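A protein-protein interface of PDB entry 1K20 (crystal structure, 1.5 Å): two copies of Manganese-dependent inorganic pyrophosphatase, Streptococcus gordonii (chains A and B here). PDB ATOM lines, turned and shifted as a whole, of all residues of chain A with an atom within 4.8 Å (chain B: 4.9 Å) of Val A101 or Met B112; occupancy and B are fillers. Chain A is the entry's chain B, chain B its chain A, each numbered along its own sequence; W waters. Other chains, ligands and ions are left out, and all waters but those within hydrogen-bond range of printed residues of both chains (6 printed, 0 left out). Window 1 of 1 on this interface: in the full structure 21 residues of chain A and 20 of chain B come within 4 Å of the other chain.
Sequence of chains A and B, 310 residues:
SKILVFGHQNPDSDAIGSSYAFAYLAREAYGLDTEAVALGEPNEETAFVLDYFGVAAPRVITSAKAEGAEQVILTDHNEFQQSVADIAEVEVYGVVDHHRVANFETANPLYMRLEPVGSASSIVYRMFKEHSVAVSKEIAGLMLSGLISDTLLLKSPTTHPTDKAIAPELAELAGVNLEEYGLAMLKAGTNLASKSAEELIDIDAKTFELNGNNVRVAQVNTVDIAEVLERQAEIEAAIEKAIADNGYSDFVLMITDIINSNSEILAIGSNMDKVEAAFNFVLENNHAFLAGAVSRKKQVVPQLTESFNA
The backbone carbonyl oxygen (O) of Thr B106 sits at hydrogen-bond distance from the guanidinium group (NH1) of Arg A100, at 3.0 Å. The backbone carbonyl oxygen (O) of Val A101 lies within hydrogen-bond range of the backbone NH (N) of Thr B106, 2.8 Å away. The backbone carbonyl oxygen of Leu A114 lies within hydrogen-bond range of the backbone NH of Met B112 (2.9 Å). The backbone NH (N) of Met A112 lies within hydrogen-bond range of the backbone carbonyl oxygen (O) of Leu B114, at 2.9 Å. The backbone carbonyl oxygen (O) of Met A112 sits close to the backbone carbonyl oxygen (O) of Met B112 (3.4 Å).
The backbone carbonyl oxygen of Tyr B111 is in hydrogen-bond range of the backbone NH of Val B95 (2.9 Å). The backbone carbonyl oxygen (O) of Val B95 lies within hydrogen-bond range of the backbone NH (N) of Arg B113 (2.9 Å). OG1 of Thr B106 lies within hydrogen-bond range of O of Asn B108 (2.7 Å). The backbone carbonyl oxygen of Arg A100 sits at hydrogen-bond distance from the side-chain amide nitrogen of Asn A78 (2.9 Å).
Among the printed residues, pairs that only touch across the chains: Arg A100 with Asn B108 (3.5 Å), Val A101 with Phe B104 (3.9 Å), Val A101 with Glu B105 (3.1 Å), Val A101 with Leu B110 (3.9 Å), Val A101 with Met B112 (3.9 Å), Met A112 with Arg B113 (3.4 Å), Arg A113 with Met B112 (3.5 Å), Leu A114 with Leu B110 (3.5 Å) and Leu A114 with Tyr B111 (3.3 Å).
Of the printed residues of chain B, Arg A100 touches Thr B106 and Asn B108. Printed residues of chain A within 4 Å of Leu B114: Met A112. Printed residues of chain A within 4 Å of Tyr B111: Leu A114 (3.3 Å). Asn A103 touches none of the printed residues of chain B. Val B95 touches none of the printed residues of chain A. The nearest printed residue of chain A that does not touch Met B112 is His A99 (6.9 Å).
Hydrophobic or aromatic side chains of chain A within 4 Å of the printed part of chain B: Val A101, Met A112 and Leu A114. Printed residues of chain B that touch a printed residue of chain A: Phe B104, Glu B105, Thr B106, Asn B108, Leu B110, Tyr B111, Met B112, Arg B113 and Leu B114. Among the printed residues, 14 pairs touch across the chains. Among the printed residues, no Asp or Glu carboxylate lies within 4 Å of a Lys or Arg side-chain nitrogen of the other chain.
Met B112 touches its own counterpart, Met A112. Met A112 touches Arg B113, and with the chains exchanged Arg A113 touches Met B112. Met A112 touches Leu B114, and with the chains exchanged Leu A114 touches Met B112. Positions printed for both chains: 104, 112, 113 and 114. Of the 14 pairs that touch across the chains among the printed residues, 5 have their exchanged pair printed and touching as well.
Water W2 bridges the backbone carbonyl oxygen of Phe B104 and the backbone carbonyl oxygen of Phe A104. Water W5 lies within hydrogen-bond range of the backbone carbonyl oxygen (O) of His A99 (2.8 Å) and the backbone NH (N) of Leu B110 (2.9 Å). Water W4 bridges the side-chain carboxylate of Glu B105 and the backbone NH of Asn A103. Water W1 bridges the backbone carbonyl oxygen of Met A112 (2.9 Å) and the backbone carbonyl oxygen of Leu B114 (3.3 Å). Water W6 bridges the backbone carbonyl oxygen (O) of Met B112 (3.0 Å) and the guanidinium group (NE) of Arg A113 (3.5 Å). Water W3 bridges the backbone carbonyl oxygen of Thr B106 (3.0 Å) and the guanidinium group of Arg A100 (3.4 Å).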
ATOM      1  N   ASN A  78       8.952  -0.968   7.610  1.00  0.00           N
ATOM      2  CA  ASN A  78      10.181  -0.197   7.749  1.00  0.00           C
ATOM      3  C   ASN A  78      10.649   0.344   6.398  1.00  0.00           C
ATOM      4  O   ASN A  78      11.272   1.399   6.336  1.00  0.00           O
ATOM      5  CB  ASN A  78      11.290  -1.028   8.421  1.00  0.00           C
ATOM      6  CG  ASN A  78      11.736  -2.209   7.587  1.00  0.00           C
ATOM      7  OD1 ASN A  78      12.613  -2.087   6.728  1.00  0.00           O
ATOM      8  ND2 ASN A  78      11.132  -3.366   7.833  1.00  0.00           N
ATOM      9  N   HIS A  99       8.757  -7.713   9.801  1.00  0.00           N
ATOM     10  CA  HIS A  99       9.092  -7.939   8.393  1.00  0.00           C
ATOM     11  C   HIS A  99      10.591  -7.874   8.140  1.00  0.00           C
ATOM     12  O   HIS A  99      11.368  -7.525   9.033  1.00  0.00           O
ATOM     13  CB  HIS A  99       8.416  -6.888   7.507  1.00  0.00           C
ATOM     14  CG  HIS A  99       6.923  -6.961   7.515  1.00  0.00           C
ATOM     15  ND1 HIS A  99       6.144  -6.239   8.394  1.00  0.00           N
ATOM     16  CD2 HIS A  99       6.068  -7.702   6.774  1.00  0.00           C
ATOM     17  CE1 HIS A  99       4.873  -6.535   8.196  1.00  0.00           C
ATOM     18  NE2 HIS A  99       4.799  -7.421   7.219  1.00  0.00           N
ATOM     19  N   ARG A 100      10.996  -8.209   6.916  1.00  0.00           N
ATOM     20  CA  ARG A 100      12.403  -8.123   6.549  1.00  0.00           C
ATOM     21  C   ARG A 100      12.744  -6.639   6.481  1.00  0.00           C
ATOM     22  O   ARG A 100      11.853  -5.795   6.337  1.00  0.00           O
ATOM     23  CB  ARG A 100      12.668  -8.796   5.188  1.00  0.00           C
ATOM     24  CG  ARG A 100      12.034  -8.136   3.949  1.00  0.00           C
ATOM     25  CD  ARG A 100      12.839  -6.944   3.411  1.00  0.00           C
ATOM     26  NE  ARG A 100      12.540  -6.671   2.002  1.00  0.00           N
ATOM     27  CZ  ARG A 100      12.956  -7.427   0.988  1.00  0.00           C
ATOM     28  NH1 ARG A 100      13.699  -8.504   1.213  1.00  0.00           N
ATOM     29  NH2 ARG A 100      12.615  -7.117  -0.257  1.00  0.00           N
ATOM     30  N   VAL A 101      14.027  -6.318   6.597  1.00  0.00           N
ATOM     31  CA  VAL A 101      14.453  -4.924   6.559  1.00  0.00           C
ATOM     32  C   VAL A 101      15.131  -4.587   5.240  1.00  0.00           C
ATOM     33  O   VAL A 101      15.956  -5.344   4.743  1.00  0.00           O
ATOM     34  CB  VAL A 101      15.427  -4.607   7.718  1.00  0.00           C
ATOM     35  CG1 VAL A 101      15.979  -3.189   7.574  1.00  0.00           C
ATOM     36  CG2 VAL A 101      14.704  -4.748   9.050  1.00  0.00           C
ATOM     37  N   ALA A 102      14.756  -3.445   4.675  1.00  0.00           N
ATOM     38  CA  ALA A 102      15.338  -2.974   3.424  1.00  0.00           C
ATOM     39  C   ALA A 102      14.888  -1.542   3.196  1.00  0.00           C
ATOM     40  O   ALA A 102      13.883  -1.106   3.759  1.00  0.00           O
ATOM     41  CB  ALA A 102      14.886  -3.855   2.255  1.00  0.00           C
ATOM     42  N   ASN A 103      15.645  -0.811   2.383  1.00  0.00           N
ATOM     43  CA  ASN A 103      15.308   0.570   2.055  1.00  0.00           C
ATOM     44  C   ASN A 103      14.944   1.373   3.293  1.00  0.00           C
ATOM     45  O   ASN A 103      13.975   2.134   3.301  1.00  0.00           O
ATOM     46  CB  ASN A 103      14.152   0.573   1.062  1.00  0.00           C
ATOM     47  CG  ASN A 103      14.454  -0.272  -0.157  1.00  0.00           C
ATOM     48  OD1 ASN A 103      15.416  -0.010  -0.876  1.00  0.00           O
ATOM     49  ND2 ASN A 103      13.648  -1.304  -0.385  1.00  0.00           N
ATOM     50  N   PHE A 104      15.746   1.198   4.334  1.00  0.00           N
ATOM     51  CA  PHE A 104      15.533   1.886   5.597  1.00  0.00           C
ATOM     52  C   PHE A 104      16.870   2.368   6.132  1.00  0.00           C
ATOM     53  O   PHE A 104      17.806   1.585   6.284  1.00  0.00           O
ATOM     54  CB  PHE A 104      14.874   0.942   6.608  1.00  0.00           C
ATOM     55  CG  PHE A 104      14.714   1.539   7.972  1.00  0.00           C
ATOM     56  CD1 PHE A 104      15.698   1.367   8.942  1.00  0.00           C
ATOM     57  CD2 PHE A 104      13.600   2.309   8.277  1.00  0.00           C
ATOM     58  CE1 PHE A 104      15.573   1.958  10.197  1.00  0.00           C
ATOM     59  CE2 PHE A 104      13.464   2.905   9.527  1.00  0.00           C
ATOM     60  CZ  PHE A 104      14.455   2.728  10.492  1.00  0.00           C
ATOM     61  N   MET A 112      14.361   0.309  17.931  1.00  0.00           N
ATOM     62  CA  MET A 112      13.828  -0.684  17.013  1.00  0.00           C
ATOM     63  C   MET A 112      13.530  -1.939  17.802  1.00  0.00           C
ATOM     64  O   MET A 112      14.342  -2.389  18.613  1.00  0.00           O
ATOM     65  CB  MET A 112      14.803  -1.034  15.887  1.00  0.00           C
ATOM     66  CG  MET A 112      15.024   0.071  14.870  1.00  0.00           C
ATOM     67  SD  MET A 112      15.957  -0.486  13.424  1.00  0.00           S
ATOM     68  CE  MET A 112      14.625  -1.042  12.362  1.00  0.00           C
ATOM     69  N   ARG A 113      12.338  -2.476  17.588  1.00  0.00           N
ATOM     70  CA  ARG A 113      11.932  -3.715  18.225  1.00  0.00           C
ATOM     71  C   ARG A 113      11.329  -4.565  17.114  1.00  0.00           C
ATOM     72  O   ARG A 113      10.169  -4.384  16.737  1.00  0.00           O
ATOM     73  CB  ARG A 113      10.899  -3.451  19.330  1.00  0.00           C
ATOM     74  CG  ARG A 113      10.403  -4.696  20.065  1.00  0.00           C
ATOM     75  CD  ARG A 113      11.509  -5.447  20.788  1.00  0.00           C
ATOM     76  NE  ARG A 113      10.980  -6.609  21.506  1.00  0.00           N
ATOM     77  CZ  ARG A 113      10.400  -6.562  22.704  1.00  0.00           C
ATOM     78  NH1 ARG A 113       9.946  -7.676  23.263  1.00  0.00           N
ATOM     79  NH2 ARG A 113      10.291  -5.412  23.357  1.00  0.00           N
ATOM     80  N   LEU A 114      12.145  -5.449  16.550  1.00  0.00           N
ATOM     81  CA  LEU A 114      11.681  -6.350  15.501  1.00  0.00           C
ATOM     82  C   LEU A 114      11.797  -7.782  15.991  1.00  0.00           C
ATOM     83  O   LEU A 114      12.765  -8.145  16.666  1.00  0.00           O
ATOM     84  CB  LEU A 114      12.498  -6.193  14.210  1.00  0.00           C
ATOM     85  CG  LEU A 114      12.019  -5.160  13.187  1.00  0.00           C
ATOM     86  CD1 LEU A 114      12.181  -3.766  13.759  1.00  0.00           C
ATOM     87  CD2 LEU A 114      12.816  -5.301  11.897  1.00  0.00           C
ATOM     88  N   VAL B  95      20.077  -8.664  15.687  1.00  0.00           N
ATOM     89  CA  VAL B  95      20.959  -7.513  15.846  1.00  0.00           C
ATOM     90  C   VAL B  95      20.629  -6.786  17.147  1.00  0.00           C
ATOM     91  O   VAL B  95      19.458  -6.570  17.456  1.00  0.00           O
ATOM     92  CB  VAL B  95      20.774  -6.477  14.699  1.00  0.00           C
ATOM     93  CG1 VAL B  95      21.698  -5.278  14.921  1.00  0.00           C
ATOM     94  CG2 VAL B  95      21.047  -7.121  13.349  1.00  0.00           C
ATOM     95  N   PHE B 104      22.053  -2.038   5.487  1.00  0.00           N
ATOM     96  CA  PHE B 104      21.611  -3.250   6.156  1.00  0.00           C
ATOM     97  C   PHE B 104      20.291  -3.709   5.557  1.00  0.00           C
ATOM     98  O   PHE B 104      19.331  -2.942   5.484  1.00  0.00           O
ATOM     99  CB  PHE B 104      21.439  -2.985   7.659  1.00  0.00           C
ATOM    100  CG  PHE B 104      20.923  -4.168   8.428  1.00  0.00           C
ATOM    101  CD1 PHE B 104      19.560  -4.329   8.659  1.00  0.00           C
ATOM    102  CD2 PHE B 104      21.797  -5.148   8.878  1.00  0.00           C
ATOM    103  CE1 PHE B 104      19.078  -5.455   9.326  1.00  0.00           C
ATOM    104  CE2 PHE B 104      21.327  -6.279   9.547  1.00  0.00           C
ATOM    105  CZ  PHE B 104      19.963  -6.432   9.771  1.00  0.00           C
ATOM    106  N   GLU B 105      20.244  -4.955   5.112  1.00  0.00           N
ATOM    107  CA  GLU B 105      19.017  -5.484   4.536  1.00  0.00           C
ATOM    108  C   GLU B 105      18.969  -6.984   4.722  1.00  0.00           C
ATOM    109  O   GLU B 105      20.006  -7.637   4.843  1.00  0.00           O
ATOM    110  CB  GLU B 105      18.925  -5.143   3.046  1.00  0.00           C
ATOM    111  CG  GLU B 105      19.990  -5.788   2.186  1.00  0.00           C
ATOM    112  CD  GLU B 105      19.911  -5.342   0.737  1.00  0.00           C
ATOM    113  OE1 GLU B 105      20.717  -5.835  -0.080  1.00  0.00           O
ATOM    114  OE2 GLU B 105      19.046  -4.497   0.417  1.00  0.00           O
ATOM    115  N   THR B 106      17.755  -7.520   4.768  1.00  0.00           N
ATOM    116  CA  THR B 106      17.562  -8.951   4.929  1.00  0.00           C
ATOM    117  C   THR B 106      16.495  -9.437   3.961  1.00  0.00           C
ATOM    118  O   THR B 106      15.674  -8.655   3.478  1.00  0.00           O
ATOM    119  CB  THR B 106      17.103  -9.313   6.361  1.00  0.00           C
ATOM    120  OG1 THR B 106      15.795  -8.773   6.597  1.00  0.00           O
ATOM    121  CG2 THR B 106      18.073  -8.754   7.394  1.00  0.00           C
ATOM    122  N   ASN B 108      14.642 -12.107   4.897  1.00  0.00           N
ATOM    123  CA  ASN B 108      13.647 -12.613   5.839  1.00  0.00           C
ATOM    124  C   ASN B 108      13.500 -11.772   7.097  1.00  0.00           C
ATOM    125  O   ASN B 108      14.351 -10.932   7.408  1.00  0.00           O
ATOM    126  CB  ASN B 108      14.051 -14.012   6.316  1.00  0.00           C
ATOM    127  CG  ASN B 108      14.266 -14.983   5.186  1.00  0.00           C
ATOM    128  OD1 ASN B 108      13.321 -15.584   4.686  1.00  0.00           O
ATOM    129  ND2 ASN B 108      15.521 -15.144   4.778  1.00  0.00           N
ATOM    130  N   LEU B 110      13.540 -10.857  11.063  1.00  0.00           N
ATOM    131  CA  LEU B 110      14.620 -11.133  12.009  1.00  0.00           C
ATOM    132  C   LEU B 110      14.349 -10.450  13.338  1.00  0.00           C
ATOM    133  O   LEU B 110      13.364  -9.725  13.497  1.00  0.00           O
ATOM    134  CB  LEU B 110      15.962 -10.604  11.474  1.00  0.00           C
ATOM    135  CG  LEU B 110      16.188  -9.087  11.589  1.00  0.00           C
ATOM    136  CD1 LEU B 110      17.675  -8.781  11.460  1.00  0.00           C
ATOM    137  CD2 LEU B 110      15.378  -8.346  10.533  1.00  0.00           C
ATOM    138  N   TYR B 111      15.243 -10.691  14.290  1.00  0.00           N
ATOM    139  CA  TYR B 111      15.178 -10.064  15.605  1.00  0.00           C
ATOM    140  C   TYR B 111      16.072  -8.829  15.591  1.00  0.00           C
ATOM    141  O   TYR B 111      17.205  -8.877  15.107  1.00  0.00           O
ATOM    142  CB  TYR B 111      15.726 -10.997  16.685  1.00  0.00           C
ATOM    143  CG  TYR B 111      14.801 -12.094  17.128  1.00  0.00           C
ATOM    144  CD1 TYR B 111      13.769 -11.840  18.030  1.00  0.00           C
ATOM    145  CD2 TYR B 111      14.962 -13.393  16.655  1.00  0.00           C
ATOM    146  CE1 TYR B 111      12.917 -12.859  18.450  1.00  0.00           C
ATOM    147  CE2 TYR B 111      14.120 -14.416  17.068  1.00  0.00           C
ATOM    148  CZ  TYR B 111      13.100 -14.142  17.964  1.00  0.00           C
ATOM    149  OH  TYR B 111      12.257 -15.155  18.365  1.00  0.00           O
ATOM    150  N   MET B 112      15.561  -7.720  16.105  1.00  0.00           N
ATOM    151  CA  MET B 112      16.360  -6.509  16.222  1.00  0.00           C
ATOM    152  C   MET B 112      15.978  -5.803  17.511  1.00  0.00           C
ATOM    153  O   MET B 112      14.797  -5.649  17.817  1.00  0.00           O
ATOM    154  CB  MET B 112      16.136  -5.543  15.056  1.00  0.00           C
ATOM    155  CG  MET B 112      16.661  -6.018  13.719  1.00  0.00           C
ATOM    156  SD  MET B 112      16.612  -4.703  12.474  1.00  0.00           S
ATOM    157  CE  MET B 112      18.237  -3.929  12.709  1.00  0.00           C
ATOM    158  N   ARG B 113      16.985  -5.413  18.281  1.00  0.00           N
ATOM    159  CA  ARG B 113      16.764  -4.665  19.507  1.00  0.00           C
ATOM    160  C   ARG B 113      17.758  -3.514  19.462  1.00  0.00           C
ATOM    161  O   ARG B 113      18.949  -3.695  19.726  1.00  0.00           O
ATOM    162  CB  ARG B 113      17.006  -5.534  20.749  1.00  0.00           C
ATOM    163  CG  ARG B 113      16.836  -4.802  22.085  1.00  0.00           C
ATOM    164  CD  ARG B 113      15.431  -4.254  22.310  1.00  0.00           C
ATOM    165  NE  ARG B 113      15.323  -3.633  23.633  1.00  0.00           N
ATOM    166  CZ  ARG B 113      15.036  -4.287  24.757  1.00  0.00           C
ATOM    167  NH1 ARG B 113      14.808  -5.595  24.741  1.00  0.00           N
ATOM    168  NH2 ARG B 113      15.005  -3.631  25.912  1.00  0.00           N
ATOM    169  N   LEU B 114      17.270  -2.346  19.062  1.00  0.00           N
ATOM    170  CA  LEU B 114      18.096  -1.150  19.001  1.00  0.00           C
ATOM    171  C   LEU B 114      17.520  -0.097  19.927  1.00  0.00           C
ATOM    172  O   LEU B 114      16.303   0.044  20.046  1.00  0.00           O
ATOM    173  CB  LEU B 114      18.156  -0.578  17.577  1.00  0.00           C
ATOM    174  CG  LEU B 114      19.244  -1.115  16.638  1.00  0.00           C
ATOM    175  CD1 LEU B 114      18.951  -2.553  16.262  1.00  0.00           C
ATOM    176  CD2 LEU B 114      19.310  -0.247  15.388  1.00  0.00           C
HETATM  177  O   HOH W   1      13.641  -1.389  21.276  1.00  0.00           O
HETATM  178  O   HOH W   2      19.721  -0.318   5.594  1.00  0.00           O
HETATM  179  O   HOH W   3      16.976  -7.581   0.976  1.00  0.00           O
HETATM  180  O   HOH W   4      18.123  -1.925   1.278  1.00  0.00           O
HETATM  181  O   HOH W   5      11.358  -8.937  11.457  1.00  0.00           O
HETATM  182  O   HOH W   6      13.913  -7.605  19.931  1.00  0.00           O
